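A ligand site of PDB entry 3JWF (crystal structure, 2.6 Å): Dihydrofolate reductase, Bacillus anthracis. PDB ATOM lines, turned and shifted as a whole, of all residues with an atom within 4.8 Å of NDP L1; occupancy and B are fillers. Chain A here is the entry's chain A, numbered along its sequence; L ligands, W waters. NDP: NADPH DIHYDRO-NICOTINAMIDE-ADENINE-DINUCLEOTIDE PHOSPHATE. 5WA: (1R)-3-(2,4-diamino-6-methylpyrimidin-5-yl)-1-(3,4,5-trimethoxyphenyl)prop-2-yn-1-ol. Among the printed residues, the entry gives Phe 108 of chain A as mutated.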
ATOM      1  N   MET A  12      15.758  32.285 -37.510  1.00  0.00           N
ATOM      2  CA  MET A  12      15.808  31.040 -38.257  1.00  0.00           C
ATOM      3  C   MET A  12      15.384  29.909 -37.341  1.00  0.00           C
ATOM      4  O   MET A  12      16.080  29.567 -36.367  1.00  0.00           O
ATOM      5  CB  MET A  12      17.211  30.802 -38.821  1.00  0.00           C
ATOM      6  CG  MET A  12      17.426  29.445 -39.490  1.00  0.00           C
ATOM      7  SD  MET A  12      16.396  29.139 -40.948  1.00  0.00           S
ATOM      8  CE  MET A  12      17.053  30.338 -42.113  1.00  0.00           C
ATOM      9  N   VAL A  13      14.222  29.325 -37.638  1.00  0.00           N
ATOM     10  CA  VAL A  13      13.618  28.342 -36.745  1.00  0.00           C
ATOM     11  C   VAL A  13      12.772  27.331 -37.503  1.00  0.00           C
ATOM     12  O   VAL A  13      12.164  27.647 -38.528  1.00  0.00           O
ATOM     13  CB  VAL A  13      12.809  29.030 -35.602  1.00  0.00           C
ATOM     14  CG1 VAL A  13      11.563  29.742 -36.140  1.00  0.00           C
ATOM     15  CG2 VAL A  13      12.451  28.036 -34.503  1.00  0.00           C
ATOM     16  N   ALA A  14      12.749  26.101 -36.984  1.00  0.00           N
ATOM     17  CA  ALA A  14      11.836  25.057 -37.423  1.00  0.00           C
ATOM     18  C   ALA A  14      11.036  24.569 -36.215  1.00  0.00           C
ATOM     19  O   ALA A  14      11.601  24.283 -35.170  1.00  0.00           O
ATOM     20  CB  ALA A  14      12.587  23.916 -38.071  1.00  0.00           C
ATOM     21  N   ILE A  21      10.368  22.896 -30.612  1.00  0.00           N
ATOM     22  CA  ILE A  21      11.623  23.023 -31.327  1.00  0.00           C
ATOM     23  C   ILE A  21      12.704  22.064 -30.812  1.00  0.00           C
ATOM     24  O   ILE A  21      13.700  21.801 -31.494  1.00  0.00           O
ATOM     25  CB  ILE A  21      12.160  24.493 -31.346  1.00  0.00           C
ATOM     26  CG1 ILE A  21      12.563  24.954 -29.937  1.00  0.00           C
ATOM     27  CG2 ILE A  21      11.152  25.457 -31.996  1.00  0.00           C
ATOM     28  CD1 ILE A  21      13.387  26.217 -29.933  1.00  0.00           C
ATOM     29  N   GLY A  22      12.501  21.513 -29.610  1.00  0.00           N
ATOM     30  CA  GLY A  22      13.499  20.645 -29.010  1.00  0.00           C
ATOM     31  C   GLY A  22      12.987  19.602 -28.039  1.00  0.00           C
ATOM     32  O   GLY A  22      11.901  19.733 -27.459  1.00  0.00           O
ATOM     33  N   LYS A  23      13.801  18.551 -27.866  1.00  0.00           N
ATOM     34  CA  LYS A  23      13.528  17.459 -26.940  1.00  0.00           C
ATOM     35  C   LYS A  23      14.845  16.914 -26.404  1.00  0.00           C
ATOM     36  O   LYS A  23      15.712  16.512 -27.179  1.00  0.00           O
ATOM     37  CB  LYS A  23      12.779  16.307 -27.629  1.00  0.00           C
ATOM     38  CG  LYS A  23      11.979  15.435 -26.668  1.00  0.00           C
ATOM     39  CD  LYS A  23      12.338  13.946 -26.770  1.00  0.00           C
ATOM     40  CE  LYS A  23      11.685  13.255 -27.962  1.00  0.00           C
ATOM     41  NZ  LYS A  23      11.827  11.760 -27.921  1.00  0.00           N
ATOM     42  N   ASN A  25      17.482  18.340 -25.210  1.00  0.00           N
ATOM     43  CA  ASN A  25      18.645  19.083 -25.737  1.00  0.00           C
ATOM     44  C   ASN A  25      19.099  18.634 -27.132  1.00  0.00           C
ATOM     45  O   ASN A  25      20.302  18.556 -27.424  1.00  0.00           O
ATOM     46  CB  ASN A  25      19.811  19.082 -24.737  1.00  0.00           C
ATOM     47  CG  ASN A  25      20.380  20.459 -24.510  1.00  0.00           C
ATOM     48  OD1 ASN A  25      19.754  21.469 -24.861  1.00  0.00           O
ATOM     49  ND2 ASN A  25      21.559  20.523 -23.903  1.00  0.00           N
ATOM     50  N   ASN A  26      18.122  18.365 -28.000  1.00  0.00           N
ATOM     51  CA  ASN A  26      18.337  17.823 -29.331  1.00  0.00           C
ATOM     52  C   ASN A  26      17.117  18.120 -30.215  1.00  0.00           C
ATOM     53  O   ASN A  26      16.078  18.552 -29.716  1.00  0.00           O
ATOM     54  CB  ASN A  26      18.500  16.310 -29.215  1.00  0.00           C
ATOM     55  CG  ASN A  26      19.418  15.706 -30.262  1.00  0.00           C
ATOM     56  OD1 ASN A  26      19.884  16.398 -31.195  1.00  0.00           O
ATOM     57  ND2 ASN A  26      19.688  14.411 -30.125  1.00  0.00           N
ATOM     58  N   LEU A  27      17.261  17.872 -31.511  1.00  0.00           N
ATOM     59  CA  LEU A  27      16.166  17.978 -32.474  1.00  0.00           C
ATOM     60  C   LEU A  27      15.288  16.735 -32.427  1.00  0.00           C
ATOM     61  O   LEU A  27      15.798  15.605 -32.465  1.00  0.00           O
ATOM     62  CB  LEU A  27      16.730  18.173 -33.877  1.00  0.00           C
ATOM     63  CG  LEU A  27      16.995  19.580 -34.463  1.00  0.00           C
ATOM     64  CD1 LEU A  27      17.166  20.691 -33.415  1.00  0.00           C
ATOM     65  CD2 LEU A  27      18.180  19.531 -35.413  1.00  0.00           C
ATOM     66  N   TRP A  29      13.361  15.667 -34.740  1.00  0.00           N
ATOM     67  CA  TRP A  29      13.216  15.132 -36.088  1.00  0.00           C
ATOM     68  C   TRP A  29      14.525  15.231 -36.867  1.00  0.00           C
ATOM     69  O   TRP A  29      15.334  16.130 -36.603  1.00  0.00           O
ATOM     70  CB  TRP A  29      12.127  15.897 -36.857  1.00  0.00           C
ATOM     71  CG  TRP A  29      12.372  17.384 -36.857  1.00  0.00           C
ATOM     72  CD1 TRP A  29      13.205  18.079 -37.687  1.00  0.00           C
ATOM     73  CD2 TRP A  29      11.804  18.351 -35.969  1.00  0.00           C
ATOM     74  NE1 TRP A  29      13.186  19.413 -37.374  1.00  0.00           N
ATOM     75  CE2 TRP A  29      12.340  19.608 -36.324  1.00  0.00           C
ATOM     76  CE3 TRP A  29      10.889  18.273 -34.911  1.00  0.00           C
ATOM     77  CZ2 TRP A  29      11.984  20.787 -35.647  1.00  0.00           C
ATOM     78  CZ3 TRP A  29      10.543  19.454 -34.236  1.00  0.00           C
ATOM     79  CH2 TRP A  29      11.090  20.686 -34.610  1.00  0.00           C
ATOM     80  N   GLY A  50      22.209  30.439 -28.425  1.00  0.00           N
ATOM     81  CA  GLY A  50      22.284  30.289 -26.973  1.00  0.00           C
ATOM     82  C   GLY A  50      23.342  29.258 -26.628  1.00  0.00           C
ATOM     83  O   GLY A  50      23.615  28.359 -27.419  1.00  0.00           O
ATOM     84  N   ARG A  51      23.931  29.384 -25.432  1.00  0.00           N
ATOM     85  CA  ARG A  51      24.992  28.477 -25.006  1.00  0.00           C
ATOM     86  C   ARG A  51      24.567  26.992 -25.106  1.00  0.00           C
ATOM     87  O   ARG A  51      25.286  26.184 -25.690  1.00  0.00           O
ATOM     88  CB  ARG A  51      25.466  28.843 -23.596  1.00  0.00           C
ATOM     89  CG  ARG A  51      26.764  28.175 -23.158  1.00  0.00           C
ATOM     90  CD  ARG A  51      26.501  26.850 -22.447  1.00  0.00           C
ATOM     91  NE  ARG A  51      25.653  27.033 -21.272  1.00  0.00           N
ATOM     92  CZ  ARG A  51      25.074  26.040 -20.601  1.00  0.00           C
ATOM     93  NH1 ARG A  51      25.241  24.776 -20.981  1.00  0.00           N
ATOM     94  NH2 ARG A  51      24.330  26.309 -19.540  1.00  0.00           N
ATOM     95  N   LYS A  52      23.395  26.673 -24.564  1.00  0.00           N
ATOM     96  CA  LYS A  52      22.881  25.303 -24.634  1.00  0.00           C
ATOM     97  C   LYS A  52      22.666  24.847 -26.082  1.00  0.00           C
ATOM     98  O   LYS A  52      23.004  23.712 -26.426  1.00  0.00           O
ATOM     99  CB  LYS A  52      21.618  25.124 -23.769  1.00  0.00           C
ATOM    100  CG  LYS A  52      21.950  24.989 -22.277  1.00  0.00           C
ATOM    101  CD  LYS A  52      20.984  24.079 -21.535  1.00  0.00           C
ATOM    102  CE  LYS A  52      19.893  24.861 -20.813  1.00  0.00           C
ATOM    103  NZ  LYS A  52      19.169  24.038 -19.798  1.00  0.00           N
ATOM    104  N   ASN A  53      22.134  25.721 -26.925  1.00  0.00           N
ATOM    105  CA  ASN A  53      22.008  25.383 -28.339  1.00  0.00           C
ATOM    106  C   ASN A  53      23.370  25.047 -28.946  1.00  0.00           C
ATOM    107  O   ASN A  53      23.495  24.051 -29.645  1.00  0.00           O
ATOM    108  CB  ASN A  53      21.288  26.468 -29.134  1.00  0.00           C
ATOM    109  CG  ASN A  53      21.118  26.121 -30.612  1.00  0.00           C
ATOM    110  OD1 ASN A  53      21.093  24.943 -30.984  1.00  0.00           O
ATOM    111  ND2 ASN A  53      21.024  27.142 -31.466  1.00  0.00           N
ATOM    112  N   VAL A  69      25.777  33.101 -26.912  1.00  0.00           N
ATOM    113  CA  VAL A  69      25.211  33.957 -25.881  1.00  0.00           C
ATOM    114  C   VAL A  69      25.138  33.222 -24.544  1.00  0.00           C
ATOM    115  O   VAL A  69      24.450  32.205 -24.422  1.00  0.00           O
ATOM    116  CB  VAL A  69      23.811  34.505 -26.276  1.00  0.00           C
ATOM    117  CG1 VAL A  69      23.253  35.424 -25.201  1.00  0.00           C
ATOM    118  CG2 VAL A  69      23.885  35.241 -27.613  1.00  0.00           C
ATOM    119  N   THR A  70      25.850  33.755 -23.553  1.00  0.00           N
ATOM    120  CA  THR A  70      25.945  33.168 -22.217  1.00  0.00           C
ATOM    121  C   THR A  70      26.152  34.261 -21.161  1.00  0.00           C
ATOM    122  O   THR A  70      26.638  35.335 -21.481  1.00  0.00           O
ATOM    123  CB  THR A  70      27.119  32.158 -22.122  1.00  0.00           C
ATOM    124  OG1 THR A  70      27.271  31.730 -20.765  1.00  0.00           O
ATOM    125  CG2 THR A  70      28.429  32.802 -22.595  1.00  0.00           C
ATOM    126  N   ARG A  71      25.781  33.969 -19.917  1.00  0.00           N
ATOM    127  CA  ARG A  71      26.046  34.880 -18.813  1.00  0.00           C
ATOM    128  C   ARG A  71      27.431  34.648 -18.203  1.00  0.00           C
ATOM    129  O   ARG A  71      27.881  35.427 -17.370  1.00  0.00           O
ATOM    130  CB  ARG A  71      24.978  34.771 -17.720  1.00  0.00           C
ATOM    131  CG  ARG A  71      23.607  35.246 -18.140  1.00  0.00           C
ATOM    132  CD  ARG A  71      22.638  35.246 -16.974  1.00  0.00           C
ATOM    133  NE  ARG A  71      21.287  35.595 -17.418  1.00  0.00           N
ATOM    134  CZ  ARG A  71      20.370  34.700 -17.790  1.00  0.00           C
ATOM    135  NH1 ARG A  71      20.646  33.404 -17.761  1.00  0.00           N
ATOM    136  NH2 ARG A  71      19.172  35.112 -18.197  1.00  0.00           N
ATOM    137  N   ASN A  72      28.083  33.561 -18.641  1.00  0.00           N
ATOM    138  CA  ASN A  72      29.416  33.171 -18.170  1.00  0.00           C
ATOM    139  C   ASN A  72      30.493  34.091 -18.739  1.00  0.00           C
ATOM    140  O   ASN A  72      30.753  34.096 -19.944  1.00  0.00           O
ATOM    141  CB  ASN A  72      29.685  31.722 -18.588  1.00  0.00           C
ATOM    142  CG  ASN A  72      30.738  31.032 -17.728  1.00  0.00           C
ATOM    143  OD1 ASN A  72      30.473  29.974 -17.157  1.00  0.00           O
ATOM    144  ND2 ASN A  72      31.937  31.606 -17.645  1.00  0.00           N
ATOM    145  N   HIS A  84      27.396  38.338 -24.252  1.00  0.00           N
ATOM    146  CA  HIS A  84      26.760  38.146 -22.935  1.00  0.00           C
ATOM    147  C   HIS A  84      25.439  38.889 -22.808  1.00  0.00           C
ATOM    148  O   HIS A  84      24.789  38.821 -21.766  1.00  0.00           O
ATOM    149  CB  HIS A  84      27.708  38.584 -21.817  1.00  0.00           C
ATOM    150  CG  HIS A  84      29.031  37.889 -21.849  1.00  0.00           C
ATOM    151  ND1 HIS A  84      30.063  38.284 -22.665  1.00  0.00           N
ATOM    152  CD2 HIS A  84      29.473  36.799 -21.180  1.00  0.00           C
ATOM    153  CE1 HIS A  84      31.097  37.484 -22.494  1.00  0.00           C
ATOM    154  NE2 HIS A  84      30.763  36.568 -21.595  1.00  0.00           N
ATOM    155  N   SER A  85      25.048  39.582 -23.879  1.00  0.00           N
ATOM    156  CA  SER A  85      23.839  40.413 -23.868  1.00  0.00           C
ATOM    157  C   SER A  85      23.383  40.730 -25.285  1.00  0.00           C
ATOM    158  O   SER A  85      24.146  40.584 -26.248  1.00  0.00           O
ATOM    159  CB  SER A  85      24.097  41.715 -23.096  1.00  0.00           C
ATOM    160  OG  SER A  85      24.934  42.587 -23.844  1.00  0.00           O
ATOM    161  N   PHE A 102      19.422  32.014 -34.056  1.00  0.00           N
ATOM    162  CA  PHE A 102      19.427  30.604 -34.405  1.00  0.00           C
ATOM    163  C   PHE A 102      18.868  29.694 -33.295  1.00  0.00           C
ATOM    164  O   PHE A 102      18.756  28.475 -33.482  1.00  0.00           O
ATOM    165  CB  PHE A 102      20.854  30.203 -34.779  1.00  0.00           C
ATOM    166  CG  PHE A 102      20.936  28.993 -35.675  1.00  0.00           C
ATOM    167  CD1 PHE A 102      20.262  28.954 -36.892  1.00  0.00           C
ATOM    168  CD2 PHE A 102      21.709  27.903 -35.299  1.00  0.00           C
ATOM    169  CE1 PHE A 102      20.349  27.842 -37.724  1.00  0.00           C
ATOM    170  CE2 PHE A 102      21.803  26.777 -36.115  1.00  0.00           C
ATOM    171  CZ  PHE A 102      21.116  26.748 -37.336  1.00  0.00           C
ATOM    172  N   GLY A 103      18.521  30.266 -32.145  1.00  0.00           N
ATOM    173  CA  GLY A 103      17.934  29.490 -31.039  1.00  0.00           C
ATOM    174  C   GLY A 103      18.878  29.207 -29.885  1.00  0.00           C
ATOM    175  O   GLY A 103      20.042  29.618 -29.916  1.00  0.00           O
ATOM    176  N   GLY A 104      18.391  28.526 -28.849  1.00  0.00           N
ATOM    177  CA  GLY A 104      17.028  28.021 -28.765  1.00  0.00           C
ATOM    178  C   GLY A 104      16.027  29.014 -28.200  1.00  0.00           C
ATOM    179  O   GLY A 104      16.061  30.194 -28.531  1.00  0.00           O
ATOM    180  N   ALA A 105      15.142  28.504 -27.344  1.00  0.00           N
ATOM    181  CA  ALA A 105      13.997  29.246 -26.851  1.00  0.00           C
ATOM    182  C   ALA A 105      14.381  30.482 -26.043  1.00  0.00           C
ATOM    183  O   ALA A 105      13.812  31.577 -26.252  1.00  0.00           O
ATOM    184  CB  ALA A 105      13.103  28.334 -26.022  1.00  0.00           C
ATOM    185  N   GLN A 106      15.331  30.317 -25.129  1.00  0.00           N
ATOM    186  CA  GLN A 106      15.764  31.411 -24.273  1.00  0.00           C
ATOM    187  C   GLN A 106      16.340  32.560 -25.098  1.00  0.00           C
ATOM    188  O   GLN A 106      16.069  33.719 -24.810  1.00  0.00           O
ATOM    189  CB  GLN A 106      16.792  30.925 -23.252  1.00  0.00           C
ATOM    190  CG  GLN A 106      16.216  29.994 -22.185  1.00  0.00           C
ATOM    191  CD  GLN A 106      17.118  29.869 -20.983  1.00  0.00           C
ATOM    192  OE1 GLN A 106      17.500  28.771 -20.587  1.00  0.00           O
ATOM    193  NE2 GLN A 106      17.474  30.994 -20.396  1.00  0.00           N
ATOM    194  N   ILE A 107      17.109  32.211 -26.120  1.00  0.00           N
ATOM    195  CA  ILE A 107      17.688  33.187 -27.040  1.00  0.00           C
ATOM    196  C   ILE A 107      16.668  33.780 -28.027  1.00  0.00           C
ATOM    197  O   ILE A 107      16.736  34.969 -28.334  1.00  0.00           O
ATOM    198  CB  ILE A 107      18.988  32.627 -27.703  1.00  0.00           C
ATOM    199  CG1 ILE A 107      20.234  33.196 -26.997  1.00  0.00           C
ATOM    200  CG2 ILE A 107      19.075  32.931 -29.175  1.00  0.00           C
ATOM    201  CD1 ILE A 107      20.303  32.928 -25.496  1.00  0.00           C
ATOM    202  N   PHE A 108      15.696  32.969 -28.470  1.00  0.00           N
ATOM    203  CA  PHE A 108      14.567  33.485 -29.265  1.00  0.00           C
ATOM    204  C   PHE A 108      13.758  34.516 -28.467  1.00  0.00           C
ATOM    205  O   PHE A 108      13.392  35.564 -29.018  1.00  0.00           O
ATOM    206  CB  PHE A 108      13.626  32.386 -29.784  1.00  0.00           C
ATOM    207  CG  PHE A 108      14.168  31.577 -30.924  1.00  0.00           C
ATOM    208  CD1 PHE A 108      13.988  30.193 -30.962  1.00  0.00           C
ATOM    209  CD2 PHE A 108      14.866  32.176 -31.974  1.00  0.00           C
ATOM    210  CE1 PHE A 108      14.499  29.438 -32.007  1.00  0.00           C
ATOM    211  CE2 PHE A 108      15.384  31.425 -33.031  1.00  0.00           C
ATOM    212  CZ  PHE A 108      15.185  30.054 -33.049  1.00  0.00           C
ATOM    213  N   LEU A 110      14.919  36.341 -25.909  1.00  0.00           N
ATOM    214  CA  LEU A 110      15.786  37.498 -25.718  1.00  0.00           C
ATOM    215  C   LEU A 110      15.711  38.507 -26.866  1.00  0.00           C
ATOM    216  O   LEU A 110      15.615  39.716 -26.635  1.00  0.00           O
ATOM    217  CB  LEU A 110      17.229  37.039 -25.516  1.00  0.00           C
ATOM    218  CG  LEU A 110      18.199  37.989 -24.817  1.00  0.00           C
ATOM    219  CD1 LEU A 110      17.650  38.518 -23.494  1.00  0.00           C
ATOM    220  CD2 LEU A 110      19.517  37.253 -24.581  1.00  0.00           C
ATOM    221  N   THR A 131      11.042  22.014 -25.350  1.00  0.00           N
ATOM    222  CA  THR A 131      11.417  23.378 -25.721  1.00  0.00           C
ATOM    223  C   THR A 131      10.548  23.920 -26.867  1.00  0.00           C
ATOM    224  O   THR A 131      10.331  23.242 -27.878  1.00  0.00           O
ATOM    225  CB  THR A 131      12.920  23.462 -26.068  1.00  0.00           C
ATOM    226  OG1 THR A 131      13.671  22.927 -24.973  1.00  0.00           O
ATOM    227  CG2 THR A 131      13.358  24.896 -26.280  1.00  0.00           C
HETATM  228  PA  NDP L   1      19.303  28.159 -25.455  1.00  0.00           P
HETATM  229  O1A NDP L   1      18.312  29.247 -25.550  1.00  0.00           O
HETATM  230  O2A NDP L   1      19.833  27.774 -26.781  1.00  0.00           O
HETATM  231  O5B NDP L   1      20.490  28.569 -24.461  1.00  0.00           O
HETATM  232  C5B NDP L   1      20.163  28.974 -23.143  1.00  0.00           C
HETATM  233  C4B NDP L   1      21.405  29.611 -22.537  1.00  0.00           C
HETATM  234  O4B NDP L   1      21.627  30.890 -23.099  1.00  0.00           O
HETATM  235  C3B NDP L   1      21.309  29.835 -21.048  1.00  0.00           C
HETATM  236  O3B NDP L   1      21.652  28.675 -20.326  1.00  0.00           O
HETATM  237  C2B NDP L   1      22.334  30.921 -20.863  1.00  0.00           C
HETATM  238  O2B NDP L   1      23.618  30.342 -20.921  1.00  0.00           O
HETATM  239  C1B NDP L   1      22.176  31.750 -22.125  1.00  0.00           C
HETATM  240  N9A NDP L   1      21.291  32.907 -21.873  1.00  0.00           N
HETATM  241  C8A NDP L   1      19.933  32.899 -21.696  1.00  0.00           C
HETATM  242  N7A NDP L   1      19.524  34.159 -21.464  1.00  0.00           N
HETATM  243  C5A NDP L   1      20.596  34.985 -21.490  1.00  0.00           C
HETATM  244  C6A NDP L   1      20.737  36.348 -21.320  1.00  0.00           C
HETATM  245  N6A NDP L   1      19.676  37.110 -21.089  1.00  0.00           N
HETATM  246  N1A NDP L   1      21.992  36.931 -21.399  1.00  0.00           N
HETATM  247  C2A NDP L   1      23.097  36.139 -21.649  1.00  0.00           C
HETATM  248  N3A NDP L   1      22.944  34.783 -21.814  1.00  0.00           N
HETATM  249  C4A NDP L   1      21.719  34.206 -21.742  1.00  0.00           C
HETATM  250  O3  NDP L   1      18.677  26.900 -24.673  1.00  0.00           O
HETATM  251  PN  NDP L   1      17.198  26.273 -24.702  1.00  0.00           P
HETATM  252  O1N NDP L   1      17.138  25.174 -23.719  1.00  0.00           O
HETATM  253  O2N NDP L   1      16.249  27.403 -24.619  1.00  0.00           O
HETATM  254  O5D NDP L   1      17.095  25.670 -26.204  1.00  0.00           O
HETATM  255  C5D NDP L   1      17.854  24.567 -26.644  1.00  0.00           C
HETATM  256  C4D NDP L   1      16.910  23.533 -27.253  1.00  0.00           C
HETATM  257  O4D NDP L   1      16.221  24.016 -28.398  1.00  0.00           O
HETATM  258  C3D NDP L   1      17.678  22.311 -27.712  1.00  0.00           C
HETATM  259  O3D NDP L   1      16.803  21.216 -27.515  1.00  0.00           O
HETATM  260  C2D NDP L   1      17.881  22.558 -29.186  1.00  0.00           C
HETATM  261  O2D NDP L   1      18.021  21.342 -29.876  1.00  0.00           O
HETATM  262  C1D NDP L   1      16.606  23.286 -29.563  1.00  0.00           C
HETATM  263  N1N NDP L   1      16.726  24.183 -30.737  1.00  0.00           N
HETATM  264  C2N NDP L   1      15.831  24.008 -31.755  1.00  0.00           C
HETATM  265  C3N NDP L   1      15.853  24.825 -32.878  1.00  0.00           C
HETATM  266  C7N NDP L   1      14.804  24.640 -33.941  1.00  0.00           C
HETATM  267  O7N NDP L   1      14.682  25.617 -34.957  1.00  0.00           O
HETATM  268  N7N NDP L   1      14.024  23.570 -33.902  1.00  0.00           N
HETATM  269  C4N NDP L   1      16.810  25.839 -32.968  1.00  0.00           C
HETATM  270  C5N NDP L   1      17.720  26.019 -31.921  1.00  0.00           C
HETATM  271  C6N NDP L   1      17.670  25.179 -30.806  1.00  0.00           C
HETATM  272  P2B NDP L   1      24.545  30.128 -19.640  1.00  0.00           P
HETATM  273  O1X NDP L   1      24.743  31.449 -18.933  1.00  0.00           O
HETATM  274  O2X NDP L   1      23.864  29.146 -18.716  1.00  0.00           O
HETATM  275  O3X NDP L   1      25.858  29.569 -20.105  1.00  0.00           O
HETATM  276  N1  5WA L   2      15.907  24.504 -38.806  1.00  0.00           N
HETATM  277  C2  5WA L   2      15.615  25.813 -38.892  1.00  0.00           C
HETATM  278  N3  5WA L   2      16.126  26.695 -38.020  1.00  0.00           N
HETATM  279  C4  5WA L   2      16.960  26.288 -37.045  1.00  0.00           C
HETATM  280  C5  5WA L   2      17.268  24.939 -36.920  1.00  0.00           C
HETATM  281  C6  5WA L   2      16.719  24.043 -37.838  1.00  0.00           C
HETATM  282  C1A 5WA L   2      22.945  22.757 -37.863  1.00  0.00           C
HETATM  283  C1B 5WA L   2      21.567  19.314 -31.839  1.00  0.00           C
HETATM  284  C1C 5WA L   2      22.218  18.313 -36.558  1.00  0.00           C
HETATM  285  C1D 5WA L   2      17.011  22.535 -37.788  1.00  0.00           C
HETATM  286  N1E 5WA L   2      14.794  26.210 -39.862  1.00  0.00           N
HETATM  287  N1F 5WA L   2      17.454  27.182 -36.188  1.00  0.00           N
HETATM  288  O1G 5WA L   2      20.642  24.739 -33.531  1.00  0.00           O
HETATM  289  C1H 5WA L   2      18.149  24.488 -35.873  1.00  0.00           C
HETATM  290  C1I 5WA L   2      18.898  24.101 -34.977  1.00  0.00           C
HETATM  291  C1J 5WA L   2      21.308  22.509 -35.617  1.00  0.00           C
HETATM  292  C1K 5WA L   2      20.769  21.317 -33.602  1.00  0.00           C
HETATM  293  O1N 5WA L   2      22.733  21.452 -37.279  1.00  0.00           O
HETATM  294  O1O 5WA L   2      21.656  19.093 -33.263  1.00  0.00           O
HETATM  295  O1P 5WA L   2      22.942  19.216 -35.697  1.00  0.00           O
HETATM  296  C1U 5WA L   2      20.654  22.464 -34.389  1.00  0.00           C
HETATM  297  C1V 5WA L   2      22.081  21.432 -36.066  1.00  0.00           C
HETATM  298  C1W 5WA L   2      21.540  20.231 -34.019  1.00  0.00           C
HETATM  299  C1X 5WA L   2      22.188  20.281 -35.267  1.00  0.00           C
HETATM  300  C1Y 5WA L   2      19.796  23.645 -33.904  1.00  0.00           C
HETATM  301  O   HOH W   1      22.912  31.917 -17.233  1.00  0.00           O
HETATM  302  O   HOH W   2      21.886  39.990 -20.356  1.00  0.00           O
HETATM  303  O   HOH W   3      27.847  28.495 -18.303  1.00  0.00           O
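Water W1 bridges an oxygen (O1X) of NDP L1 and the guanidinium group of Arg 71. Water W3 bridges O3X of NDP L1 (2.9 Å) and OD1 of Asn 72 (3.2 Å). Water W2 bridges N1A of NDP L1 (3.2 Å) and O of His 84 (3.4 Å).
The side-chain hydroxyl (OG1) of Thr 70 lies within hydrogen-bond range of the backbone NH (N) of Asn 72 (2.9 Å). The backbone NH of Arg 51 lies within hydrogen-bond range of the backbone carbonyl oxygen of Val 69 (3.0 Å). N of Ile 21 lies within hydrogen-bond range of O of Thr 131 (2.8 Å). The side-chain amide nitrogen (ND2) of Asn 53 lies within hydrogen-bond range of the backbone carbonyl oxygen (O) of Phe 102 (3.3 Å). ND2 of Asn 53 sits at hydrogen-bond distance from O of Gly 103, at 3.1 Å. A ring nitrogen (NE2) of His 84 sits at hydrogen-bond distance from the backbone carbonyl oxygen (O) of Asn 72, at 3.0 Å. N of Gly 50 sits at hydrogen-bond distance from O of Gly 103. O of Gly 22 is in hydrogen-bond range of N of Thr 131 (3.2 Å).
An oxygen (O7N) of NDP L1 sits close to a nitrogen (N1F) of 5WA L2 (3.4 Å).
O of Val 69 sits close to O4B of NDP L1, 3.4 Å away. O of His 84 sits close to N1A of NDP L1. Merely in contact with NDP L1: Phe 102, Val 13, Asn 25, Leu 110, Gly 50, Gly 103, Thr 131, Gly 22, Leu 27, Trp 29 and Asn 72. Within 4 Å of NDP L1: Val 13, Ala 14, Ile 21, Gly 22, Asn 25, Asn 26, Leu 27, Trp 29, Gly 50, Arg 51, Lys 52, Asn 53, Val 69, Thr 70, Arg 71, Asn 72, His 84, Phe 102, Gly 103, Gly 104, Ala 105, Gln 106, Ile 107, Leu 110 and Thr 131.
N of Gly 104 is in hydrogen-bond range of O2A of NDP L1. OG1 of Thr 70 lies within hydrogen-bond range of O3X of NDP L1, at 2.7 Å. The guanidinium group of Arg 51 lies within salt-bridge range of an oxygen (O3X) of NDP L1 (2.8 Å). An oxygen (O7N) of NDP L1 lies within hydrogen-bond range of the backbone NH (N) of Ala 14, at 2.8 Å. The backbone carbonyl oxygen (O) of Ala 14 sits at hydrogen-bond distance from a nitrogen (N7N) of NDP L1, 2.8 Å away. The backbone NH (N) of Arg 71 sits at hydrogen-bond distance from an oxygen (O1X) of NDP L1. N7A of NDP L1 is in hydrogen-bond range of NH2 of Arg 71 (3.4 Å). The backbone carbonyl oxygen (O) of Ile 21 is in hydrogen-bond range of a nitrogen (N7N) of NDP L1 (3.0 Å). The backbone NH (N) of Asn 53 sits close to an oxygen (O2A) of NDP L1 (3.1 Å). The backbone NH of Gln 106 sits at hydrogen-bond distance from an oxygen (O2N) of NDP L1 (3.1 Å). N of Ala 105 lies within hydrogen-bond range of O2N of NDP L1. N of Asn 26 sits at hydrogen-bond distance from O3D of NDP L1 (3.2 Å). The backbone carbonyl oxygen of Asn 26 sits close to an oxygen (O2D) of NDP L1 (3.4 Å). An oxygen (O1A) of NDP L1 sits at hydrogen-bond distance from the backbone NH (N) of Ile 107 (3.2 Å). The backbone NH (N) of Lys 52 is in hydrogen-bond range of an oxygen (O5B) of NDP L1. The side-chain amide oxygen of Asn 53 lies within hydrogen-bond range of an oxygen (O1G) of 5WA L2 (2.6 Å). The backbone carbonyl oxygen (O) of Phe 102 sits at hydrogen-bond distance from a nitrogen (N1F) of 5WA L2 (3.3 Å). A nitrogen (N3) of 5WA L2 sits close to the backbone NH (N) of Val 13, 3.3 Å away. The backbone carbonyl oxygen (O) of Val 13 is in hydrogen-bond range of a nitrogen (N1E) of 5WA L2 (3.3 Å). The backbone carbonyl oxygen (O) of Met 12 sits at hydrogen-bond distance from a nitrogen (N1F) of 5WA L2 (2.8 Å). The side-chain sulfur of Met 12 is in hydrogen-bond range of a nitrogen (N1E) of 5WA L2 (3.5 Å).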
